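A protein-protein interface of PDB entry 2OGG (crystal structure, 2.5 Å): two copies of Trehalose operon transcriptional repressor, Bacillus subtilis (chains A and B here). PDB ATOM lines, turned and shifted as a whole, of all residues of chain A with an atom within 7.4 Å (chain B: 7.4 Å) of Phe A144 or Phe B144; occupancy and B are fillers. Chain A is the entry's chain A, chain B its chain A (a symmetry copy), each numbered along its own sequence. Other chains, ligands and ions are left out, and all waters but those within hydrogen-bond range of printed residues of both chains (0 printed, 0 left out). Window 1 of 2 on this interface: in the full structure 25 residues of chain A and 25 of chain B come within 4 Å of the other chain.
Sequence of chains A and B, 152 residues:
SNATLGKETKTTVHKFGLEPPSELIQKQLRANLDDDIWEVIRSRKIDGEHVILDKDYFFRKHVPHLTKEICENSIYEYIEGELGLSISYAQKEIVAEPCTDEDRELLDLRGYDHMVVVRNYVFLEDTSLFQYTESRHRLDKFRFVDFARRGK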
ATOM      1  N   LYS A  92     -13.104  38.149  13.807  1.00  0.00           N
ATOM      2  CA  LYS A  92     -12.557  36.817  13.544  1.00  0.00           C
ATOM      3  C   LYS A  92     -13.113  36.256  12.232  1.00  0.00           C
ATOM      4  O   LYS A  92     -14.304  36.363  11.957  1.00  0.00           O
ATOM      5  CB  LYS A  92     -12.988  35.896  14.686  1.00  0.00           C
ATOM      6  CG  LYS A  92     -11.999  34.862  15.078  1.00  0.00           C
ATOM      7  CD  LYS A  92     -12.274  34.336  16.494  1.00  0.00           C
ATOM      8  CE  LYS A  92     -11.574  35.189  17.565  1.00  0.00           C
ATOM      9  NZ  LYS A  92     -11.975  34.831  18.976  1.00  0.00           N
ATOM     10  N   GLU A  93     -12.269  35.629  11.425  1.00  0.00           N
ATOM     11  CA  GLU A  93     -12.751  34.968  10.236  1.00  0.00           C
ATOM     12  C   GLU A  93     -12.063  33.608  10.186  1.00  0.00           C
ATOM     13  O   GLU A  93     -10.833  33.523  10.332  1.00  0.00           O
ATOM     14  CB  GLU A  93     -12.417  35.782   8.985  1.00  0.00           C
ATOM     15  CG  GLU A  93     -13.007  35.166   7.699  1.00  0.00           C
ATOM     16  CD  GLU A  93     -12.276  35.566   6.415  1.00  0.00           C
ATOM     17  OE1 GLU A  93     -11.019  35.615   6.418  1.00  0.00           O
ATOM     18  OE2 GLU A  93     -12.950  35.646   5.361  1.00  0.00           O
ATOM     19  N   ILE A  94     -12.877  32.551  10.199  1.00  0.00           N
ATOM     20  CA  ILE A  94     -12.389  31.169  10.235  1.00  0.00           C
ATOM     21  C   ILE A  94     -12.745  30.462   8.929  1.00  0.00           C
ATOM     22  O   ILE A  94     -13.916  30.334   8.583  1.00  0.00           O
ATOM     23  CB  ILE A  94     -13.054  30.371  11.381  1.00  0.00           C
ATOM     24  CG1 ILE A  94     -12.815  31.040  12.727  1.00  0.00           C
ATOM     25  CG2 ILE A  94     -12.499  28.987  11.457  1.00  0.00           C
ATOM     26  CD1 ILE A  94     -13.645  30.460  13.786  1.00  0.00           C
ATOM     27  N   VAL A  95     -11.734  30.047   8.189  1.00  0.00           N
ATOM     28  CA  VAL A  95     -11.939  29.295   6.953  1.00  0.00           C
ATOM     29  C   VAL A  95     -11.000  28.087   6.906  1.00  0.00           C
ATOM     30  O   VAL A  95     -10.273  27.812   7.869  1.00  0.00           O
ATOM     31  CB  VAL A  95     -11.625  30.158   5.713  1.00  0.00           C
ATOM     32  CG1 VAL A  95     -12.490  31.403   5.697  1.00  0.00           C
ATOM     33  CG2 VAL A  95     -10.148  30.534   5.712  1.00  0.00           C
ATOM     34  N   VAL A 116      -7.279  24.407   9.304  1.00  0.00           N
ATOM     35  CA  VAL A 116      -8.278  25.361   9.726  1.00  0.00           C
ATOM     36  C   VAL A 116      -7.522  26.659  10.073  1.00  0.00           C
ATOM     37  O   VAL A 116      -6.455  26.592  10.692  1.00  0.00           O
ATOM     38  CB  VAL A 116      -9.109  24.827  10.916  1.00  0.00           C
ATOM     39  CG1 VAL A 116     -10.105  25.913  11.432  1.00  0.00           C
ATOM     40  CG2 VAL A 116      -9.872  23.619  10.497  1.00  0.00           C
ATOM     41  N   VAL A 117      -7.883  27.750   9.395  1.00  0.00           N
ATOM     42  CA  VAL A 117      -7.188  29.021   9.576  1.00  0.00           C
ATOM     43  C   VAL A 117      -8.055  30.074  10.244  1.00  0.00           C
ATOM     44  O   VAL A 117      -9.071  30.506   9.691  1.00  0.00           O
ATOM     45  CB  VAL A 117      -6.662  29.618   8.262  1.00  0.00           C
ATOM     46  CG1 VAL A 117      -5.942  30.936   8.552  1.00  0.00           C
ATOM     47  CG2 VAL A 117      -5.728  28.648   7.558  1.00  0.00           C
ATOM     48  N   VAL A 118      -7.689  30.429  11.467  1.00  0.00           N
ATOM     49  CA  VAL A 118      -8.373  31.490  12.201  1.00  0.00           C
ATOM     50  C   VAL A 118      -7.631  32.815  12.066  1.00  0.00           C
ATOM     51  O   VAL A 118      -6.438  32.926  12.389  1.00  0.00           O
ATOM     52  CB  VAL A 118      -8.507  31.145  13.693  1.00  0.00           C
ATOM     53  CG1 VAL A 118      -9.297  32.238  14.392  1.00  0.00           C
ATOM     54  CG2 VAL A 118      -9.186  29.770  13.858  1.00  0.00           C
ATOM     55  N   ARG A 119      -8.322  33.791  11.492  1.00  0.00           N
ATOM     56  CA  ARG A 119      -7.774  35.134  11.354  1.00  0.00           C
ATOM     57  C   ARG A 119      -8.515  36.100  12.237  1.00  0.00           C
ATOM     58  O   ARG A 119      -9.729  36.227  12.144  1.00  0.00           O
ATOM     59  CB  ARG A 119      -7.865  35.607   9.922  1.00  0.00           C
ATOM     60  CG  ARG A 119      -6.809  34.997   9.041  1.00  0.00           C
ATOM     61  CD  ARG A 119      -6.964  35.522   7.633  1.00  0.00           C
ATOM     62  NE  ARG A 119      -5.975  34.957   6.729  1.00  0.00           N
ATOM     63  CZ  ARG A 119      -6.183  33.897   5.956  1.00  0.00           C
ATOM     64  NH1 ARG A 119      -7.277  33.149   6.090  1.00  0.00           N
ATOM     65  NH2 ARG A 119      -5.206  33.477   5.194  1.00  0.00           N
ATOM     66  N   PHE A 142      -8.421  21.332  15.958  1.00  0.00           N
ATOM     67  CA  PHE A 142      -9.143  22.570  15.931  1.00  0.00           C
ATOM     68  C   PHE A 142     -10.460  22.378  16.645  1.00  0.00           C
ATOM     69  O   PHE A 142     -11.114  21.358  16.444  1.00  0.00           O
ATOM     70  CB  PHE A 142      -9.399  23.007  14.493  1.00  0.00           C
ATOM     71  CG  PHE A 142     -10.185  24.261  14.404  1.00  0.00           C
ATOM     72  CD1 PHE A 142      -9.621  25.446  14.812  1.00  0.00           C
ATOM     73  CD2 PHE A 142     -11.558  24.211  14.213  1.00  0.00           C
ATOM     74  CE1 PHE A 142     -10.390  26.614  14.880  1.00  0.00           C
ATOM     75  CE2 PHE A 142     -12.339  25.352  14.330  1.00  0.00           C
ATOM     76  CZ  PHE A 142     -11.755  26.556  14.649  1.00  0.00           C
ATOM     77  N   ARG A 143     -10.727  23.233  17.627  1.00  0.00           N
ATOM     78  CA  ARG A 143     -12.029  23.255  18.274  1.00  0.00           C
ATOM     79  C   ARG A 143     -12.323  24.668  18.706  1.00  0.00           C
ATOM     80  O   ARG A 143     -11.474  25.312  19.274  1.00  0.00           O
ATOM     81  CB  ARG A 143     -12.064  22.326  19.479  1.00  0.00           C
ATOM     82  CG  ARG A 143     -13.374  22.362  20.277  1.00  0.00           C
ATOM     83  CD  ARG A 143     -13.388  21.264  21.349  1.00  0.00           C
ATOM     84  NE  ARG A 143     -14.571  21.319  22.202  1.00  0.00           N
ATOM     85  CZ  ARG A 143     -14.652  21.996  23.353  1.00  0.00           C
ATOM     86  NH1 ARG A 143     -13.607  22.673  23.821  1.00  0.00           N
ATOM     87  NH2 ARG A 143     -15.791  22.000  24.036  1.00  0.00           N
ATOM     88  N   PHE A 144     -13.428  25.222  18.233  1.00  0.00           N
ATOM     89  CA  PHE A 144     -13.787  26.584  18.566  1.00  0.00           C
ATOM     90  C   PHE A 144     -15.156  26.616  19.216  1.00  0.00           C
ATOM     91  O   PHE A 144     -16.097  25.995  18.701  1.00  0.00           O
ATOM     92  CB  PHE A 144     -13.804  27.415  17.310  1.00  0.00           C
ATOM     93  CG  PHE A 144     -14.347  28.788  17.506  1.00  0.00           C
ATOM     94  CD1 PHE A 144     -13.486  29.872  17.623  1.00  0.00           C
ATOM     95  CD2 PHE A 144     -15.717  29.015  17.488  1.00  0.00           C
ATOM     96  CE1 PHE A 144     -13.984  31.154  17.760  1.00  0.00           C
ATOM     97  CE2 PHE A 144     -16.217  30.297  17.539  1.00  0.00           C
ATOM     98  CZ  PHE A 144     -15.352  31.370  17.721  1.00  0.00           C
ATOM     99  N   VAL A 145     -15.210  27.157  20.429  1.00  0.00           N
ATOM    100  CA  VAL A 145     -16.439  27.295  21.173  1.00  0.00           C
ATOM    101  C   VAL A 145     -16.821  28.753  21.335  1.00  0.00           C
ATOM    102  O   VAL A 145     -15.963  29.625  21.323  1.00  0.00           O
ATOM    103  CB  VAL A 145     -16.289  26.702  22.551  1.00  0.00           C
ATOM    104  CG1 VAL A 145     -17.653  26.653  23.258  1.00  0.00           C
ATOM    105  CG2 VAL A 145     -15.739  25.310  22.431  1.00  0.00           C
ATOM    106  N   ASP A 146     -18.119  29.029  21.398  1.00  0.00           N
ATOM    107  CA  ASP A 146     -18.583  30.379  21.682  1.00  0.00           C
ATOM    108  C   ASP A 146     -20.069  30.467  21.977  1.00  0.00           C
ATOM    109  O   ASP A 146     -20.713  29.464  22.266  1.00  0.00           O
ATOM    110  CB  ASP A 146     -18.224  31.334  20.546  1.00  0.00           C
ATOM    111  CG  ASP A 146     -18.030  32.768  21.028  1.00  0.00           C
ATOM    112  OD1 ASP A 146     -17.369  33.577  20.270  1.00  0.00           O
ATOM    113  OD2 ASP A 146     -18.472  33.075  22.184  1.00  0.00           O
ATOM    114  N   PHE A 147     -20.461  31.690  22.293  1.00  0.00           N
ATOM    115  CA  PHE A 147     -21.845  32.135  22.243  1.00  0.00           C
ATOM    116  C   PHE A 147     -21.691  33.369  21.355  1.00  0.00           C
ATOM    117  O   PHE A 147     -20.554  33.733  21.034  1.00  0.00           O
ATOM    118  CB  PHE A 147     -22.308  32.547  23.643  1.00  0.00           C
ATOM    119  CG  PHE A 147     -21.794  31.661  24.735  1.00  0.00           C
ATOM    120  CD1 PHE A 147     -20.539  31.863  25.269  1.00  0.00           C
ATOM    121  CD2 PHE A 147     -22.614  30.718  25.315  1.00  0.00           C
ATOM    122  CE1 PHE A 147     -20.070  31.068  26.301  1.00  0.00           C
ATOM    123  CE2 PHE A 147     -22.163  29.913  26.349  1.00  0.00           C
ATOM    124  CZ  PHE A 147     -20.880  30.079  26.833  1.00  0.00           C
ATOM    125  N   LYS B  92     -22.070  27.303  20.504  1.00  0.00           N
ATOM    126  CA  LYS B  92     -21.561  26.809  19.224  1.00  0.00           C
ATOM    127  C   LYS B  92     -20.243  26.054  19.424  1.00  0.00           C
ATOM    128  O   LYS B  92     -19.371  26.496  20.163  1.00  0.00           O
ATOM    129  CB  LYS B  92     -21.295  28.016  18.324  1.00  0.00           C
ATOM    130  CG  LYS B  92     -21.565  27.806  16.880  1.00  0.00           C
ATOM    131  CD  LYS B  92     -21.758  29.141  16.149  1.00  0.00           C
ATOM    132  CE  LYS B  92     -23.222  29.610  16.193  1.00  0.00           C
ATOM    133  NZ  LYS B  92     -23.423  31.008  15.662  1.00  0.00           N
ATOM    134  N   GLU B  93     -20.073  24.927  18.748  1.00  0.00           N
ATOM    135  CA  GLU B  93     -18.808  24.234  18.792  1.00  0.00           C
ATOM    136  C   GLU B  93     -18.479  23.837  17.358  1.00  0.00           C
ATOM    137  O   GLU B  93     -19.329  23.264  16.657  1.00  0.00           O
ATOM    138  CB  GLU B  93     -18.895  22.994  19.684  1.00  0.00           C
ATOM    139  CG  GLU B  93     -17.536  22.281  19.846  1.00  0.00           C
ATOM    140  CD  GLU B  93     -17.641  20.799  20.217  1.00  0.00           C
ATOM    141  OE1 GLU B  93     -18.516  20.091  19.656  1.00  0.00           O
ATOM    142  OE2 GLU B  93     -16.730  20.308  20.923  1.00  0.00           O
ATOM    143  N   ILE B  94     -17.340  24.332  16.871  1.00  0.00           N
ATOM    144  CA  ILE B  94     -16.905  24.119  15.487  1.00  0.00           C
ATOM    145  C   ILE B  94     -15.643  23.259  15.468  1.00  0.00           C
ATOM    146  O   ILE B  94     -14.617  23.638  16.026  1.00  0.00           O
ATOM    147  CB  ILE B  94     -16.553  25.459  14.798  1.00  0.00           C
ATOM    148  CG1 ILE B  94     -17.734  26.418  14.828  1.00  0.00           C
ATOM    149  CG2 ILE B  94     -16.182  25.241  13.368  1.00  0.00           C
ATOM    150  CD1 ILE B  94     -17.353  27.775  14.425  1.00  0.00           C
ATOM    151  N   VAL B  95     -15.736  22.088  14.868  1.00  0.00           N
ATOM    152  CA  VAL B  95     -14.583  21.202  14.719  1.00  0.00           C
ATOM    153  C   VAL B  95     -14.511  20.662  13.289  1.00  0.00           C
ATOM    154  O   VAL B  95     -15.304  21.052  12.424  1.00  0.00           O
ATOM    155  CB  VAL B  95     -14.691  19.981  15.658  1.00  0.00           C
ATOM    156  CG1 VAL B  95     -14.803  20.427  17.102  1.00  0.00           C
ATOM    157  CG2 VAL B  95     -15.897  19.137  15.263  1.00  0.00           C
ATOM    158  N   VAL B 116     -16.082  20.626   7.751  1.00  0.00           N
ATOM    159  CA  VAL B 116     -16.150  21.515   8.887  1.00  0.00           C
ATOM    160  C   VAL B 116     -17.558  21.344   9.492  1.00  0.00           C
ATOM    161  O   VAL B 116     -18.534  21.254   8.740  1.00  0.00           O
ATOM    162  CB  VAL B 116     -15.857  22.979   8.483  1.00  0.00           C
ATOM    163  CG1 VAL B 116     -16.046  23.942   9.698  1.00  0.00           C
ATOM    164  CG2 VAL B 116     -14.461  23.093   7.977  1.00  0.00           C
ATOM    165  N   VAL B 117     -17.607  20.963  10.770  1.00  0.00           N
ATOM    166  CA  VAL B 117     -18.879  20.689  11.432  1.00  0.00           C
ATOM    167  C   VAL B 117     -19.209  21.705  12.512  1.00  0.00           C
ATOM    168  O   VAL B 117     -18.505  21.812  13.521  1.00  0.00           O
ATOM    169  CB  VAL B 117     -18.944  19.294  12.071  1.00  0.00           C
ATOM    170  CG1 VAL B 117     -20.311  19.095  12.727  1.00  0.00           C
ATOM    171  CG2 VAL B 117     -18.689  18.209  11.039  1.00  0.00           C
ATOM    172  N   VAL B 118     -20.239  22.499  12.260  1.00  0.00           N
ATOM    173  CA  VAL B 118     -20.728  23.465  13.239  1.00  0.00           C
ATOM    174  C   VAL B 118     -21.912  22.903  14.019  1.00  0.00           C
ATOM    175  O   VAL B 118     -22.933  22.493  13.443  1.00  0.00           O
ATOM    176  CB  VAL B 118     -21.155  24.779  12.567  1.00  0.00           C
ATOM    177  CG1 VAL B 118     -21.575  25.777  13.633  1.00  0.00           C
ATOM    178  CG2 VAL B 118     -20.000  25.332  11.707  1.00  0.00           C
ATOM    179  N   ARG B 119     -21.724  22.796  15.328  1.00  0.00           N
ATOM    180  CA  ARG B 119     -22.786  22.341  16.216  1.00  0.00           C
ATOM    181  C   ARG B 119     -23.254  23.466  17.099  1.00  0.00           C
ATOM    182  O   ARG B 119     -22.463  24.071  17.812  1.00  0.00           O
ATOM    183  CB  ARG B 119     -22.308  21.200  17.084  1.00  0.00           C
ATOM    184  CG  ARG B 119     -22.254  19.892  16.343  1.00  0.00           C
ATOM    185  CD  ARG B 119     -21.774  18.805  17.276  1.00  0.00           C
ATOM    186  NE  ARG B 119     -21.689  17.514  16.612  1.00  0.00           N
ATOM    187  CZ  ARG B 119     -20.583  17.019  16.071  1.00  0.00           C
ATOM    188  NH1 ARG B 119     -19.487  17.765  15.936  1.00  0.00           N
ATOM    189  NH2 ARG B 119     -20.640  15.849  15.489  1.00  0.00           N
ATOM    190  N   PHE B 142     -16.753  26.834   3.745  1.00  0.00           N
ATOM    191  CA  PHE B 142     -16.953  27.190   5.119  1.00  0.00           C
ATOM    192  C   PHE B 142     -16.298  28.527   5.373  1.00  0.00           C
ATOM    193  O   PHE B 142     -15.187  28.755   4.904  1.00  0.00           O
ATOM    194  CB  PHE B 142     -16.341  26.138   6.036  1.00  0.00           C
ATOM    195  CG  PHE B 142     -16.477  26.478   7.474  1.00  0.00           C
ATOM    196  CD1 PHE B 142     -17.721  26.468   8.058  1.00  0.00           C
ATOM    197  CD2 PHE B 142     -15.433  27.096   8.145  1.00  0.00           C
ATOM    198  CE1 PHE B 142     -17.896  26.930   9.368  1.00  0.00           C
ATOM    199  CE2 PHE B 142     -15.608  27.608   9.424  1.00  0.00           C
ATOM    200  CZ  PHE B 142     -16.833  27.512  10.041  1.00  0.00           C
ATOM    201  N   ARG B 143     -17.070  29.467   5.908  1.00  0.00           N
ATOM    202  CA  ARG B 143     -16.515  30.736   6.351  1.00  0.00           C
ATOM    203  C   ARG B 143     -17.321  31.225   7.526  1.00  0.00           C
ATOM    204  O   ARG B 143     -18.527  31.198   7.480  1.00  0.00           O
ATOM    205  CB  ARG B 143     -16.542  31.771   5.236  1.00  0.00           C
ATOM    206  CG  ARG B 143     -16.060  33.168   5.649  1.00  0.00           C
ATOM    207  CD  ARG B 143     -15.943  34.087   4.426  1.00  0.00           C
ATOM    208  NE  ARG B 143     -15.585  35.457   4.778  1.00  0.00           N
ATOM    209  CZ  ARG B 143     -16.461  36.436   5.026  1.00  0.00           C
ATOM    210  NH1 ARG B 143     -17.771  36.217   4.944  1.00  0.00           N
ATOM    211  NH2 ARG B 143     -16.023  37.643   5.366  1.00  0.00           N
ATOM    212  N   PHE B 144     -16.664  31.445   8.654  1.00  0.00           N
ATOM    213  CA  PHE B 144     -17.351  31.890   9.848  1.00  0.00           C
ATOM    214  C   PHE B 144     -16.757  33.198  10.331  1.00  0.00           C
ATOM    215  O   PHE B 144     -15.527  33.320  10.423  1.00  0.00           O
ATOM    216  CB  PHE B 144     -17.209  30.844  10.922  1.00  0.00           C
ATOM    217  CG  PHE B 144     -17.712  31.279  12.254  1.00  0.00           C
ATOM    218  CD1 PHE B 144     -18.960  30.864  12.702  1.00  0.00           C
ATOM    219  CD2 PHE B 144     -16.909  32.033  13.101  1.00  0.00           C
ATOM    220  CE1 PHE B 144     -19.414  31.228  13.956  1.00  0.00           C
ATOM    221  CE2 PHE B 144     -17.321  32.327  14.382  1.00  0.00           C
ATOM    222  CZ  PHE B 144     -18.596  31.963  14.799  1.00  0.00           C
ATOM    223  N   VAL B 145     -17.605  34.217  10.435  1.00  0.00           N
ATOM    224  CA  VAL B 145     -17.211  35.521  10.911  1.00  0.00           C
ATOM    225  C   VAL B 145     -17.854  35.835  12.246  1.00  0.00           C
ATOM    226  O   VAL B 145     -18.919  35.321  12.560  1.00  0.00           O
ATOM    227  CB  VAL B 145     -17.634  36.588   9.933  1.00  0.00           C
ATOM    228  CG1 VAL B 145     -17.026  37.943  10.329  1.00  0.00           C
ATOM    229  CG2 VAL B 145     -17.161  36.211   8.558  1.00  0.00           C
ATOM    230  N   ASP B 146     -17.165  36.615  13.074  1.00  0.00           N
ATOM    231  CA  ASP B 146     -17.752  37.078  14.324  1.00  0.00           C
ATOM    232  C   ASP B 146     -16.942  38.159  15.016  1.00  0.00           C
ATOM    233  O   ASP B 146     -16.080  38.785  14.408  1.00  0.00           O
ATOM    234  CB  ASP B 146     -17.991  35.916  15.284  1.00  0.00           C
ATOM    235  CG  ASP B 146     -19.161  36.169  16.228  1.00  0.00           C
ATOM    236  OD1 ASP B 146     -19.701  35.152  16.810  1.00  0.00           O
ATOM    237  OD2 ASP B 146     -19.588  37.366  16.343  1.00  0.00           O
ATOM    238  N   PHE B 147     -17.518  38.612  16.117  1.00  0.00           N
ATOM    239  CA  PHE B 147     -16.814  39.341  17.159  1.00  0.00           C
ATOM    240  C   PHE B 147     -17.191  38.493  18.373  1.00  0.00           C
ATOM    241  O   PHE B 147     -18.009  37.577  18.228  1.00  0.00           O
ATOM    242  CB  PHE B 147     -17.403  40.748  17.296  1.00  0.00           C
ATOM    243  CG  PHE B 147     -17.770  41.380  15.989  1.00  0.00           C
ATOM    244  CD1 PHE B 147     -18.984  41.107  15.394  1.00  0.00           C
ATOM    245  CD2 PHE B 147     -16.962  42.344  15.426  1.00  0.00           C
ATOM    246  CE1 PHE B 147     -19.343  41.712  14.203  1.00  0.00           C
ATOM    247  CE2 PHE B 147     -17.305  42.961  14.234  1.00  0.00           C
ATOM    248  CZ  PHE B 147     -18.494  42.632  13.613  1.00  0.00           C
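O of Phe B144 lies within hydrogen-bond range of N of Ile A94. The guanidinium group (NE) of Arg A143 is in salt-bridge range of the side-chain carboxylate (OE2) of Glu B93 (2.7 Å). N of Ile B94 sits at hydrogen-bond distance from O of Phe A144. The backbone carbonyl oxygen (O) of Lys B92 is in hydrogen-bond range of the backbone NH (N) of Asp A146, 3.1 Å away. NE of Arg B143 is in salt-bridge range of OE2 of Glu A93 (2.7 Å). O of Lys A92 lies within hydrogen-bond range of N of Asp B146.
Printed residues of chain B within 4 Å of Glu A93: Arg B143 (2.7 Å) and Phe B144 (3.2 Å). Of the printed residues of chain B, Ile A94 touches Phe B142 (3.3 Å), Arg B143 (3.4 Å) and Phe B144 (2.8 Å). Val A116 touches none of the printed residues of chain B. Of the printed residues of chain B, Arg A143 touches Glu B93 (2.7 Å), Ile B94 (3.4 Å) and Val B95 (3.98 Å). Of chain B, only Lys B92 (3.6 Å), Glu B93 (3.2 Å), Ile B94 (2.8 Å) and Phe B144 (3.9 Å) come within 4 Å of Phe A144. Of the printed residues of chain A, Arg B143 touches Glu A93, Ile A94 and Val A95. Phe B144 touches just these residues of chain A: Lys A92, Glu A93, Ile A94 and Phe A144. The nearest residue of chain A that does not touch Phe B144 is Val A95 (5.1 Å).
Lys A92 touches Phe B144. O of Ile A94 touches CE2 of Phe B142, 3.3 Å away. CA of Arg B143 touches O of Ile A94, at 3.4 Å. O of Phe B142 touches CG1 of Val A95, 3.9 Å away. Arg B143 touches Val A95 (CG to CG1, 3.98 Å). CE2 of Phe A142 touches O of Ile B94 (3.3 Å). O of Phe A142 touches CG1 of Val B95, at 3.9 Å. Val B95 touches Arg A143. Lys B92 touches Phe A144. Lys B92 touches Val A145.
The backbone NH (N) of Glu B93 sits at hydrogen-bond distance from the backbone carbonyl oxygen (O) of Arg B119, at 2.7 Å. O of Val A95 sits at hydrogen-bond distance from N of Val A117. O of Arg A119 is in hydrogen-bond range of N of Glu A93. N of Val B117 sits at hydrogen-bond distance from O of Val B95 (2.8 Å).
Of the 14 printed residues of chain B, 9 touch a printed residue of chain A. Hydrophobic or aromatic side chains of chain A that line the printed part of chain B: Ile A94, Val A95, Phe A142, Phe A144 and Val A145. Among the printed residues, 21 pairs touch across the chains. Among the printed residues, Asp or Glu carboxylates within 4 Å of a Lys or Arg side-chain nitrogen of the other chain: Glu A93 with Arg B143 and Arg A143 with Glu B93.
Lys A92 touches Phe B144, and with the chains exchanged Phe A144 touches Lys B92. Glu A93 touches Phe B144, and with the chains exchanged Phe A144 touches Glu B93. Val A95 touches Phe B142, and with the chains exchanged Phe A142 touches Val B95. Val A95 touches Arg B143, and with the chains exchanged Arg A143 touches Val B95.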
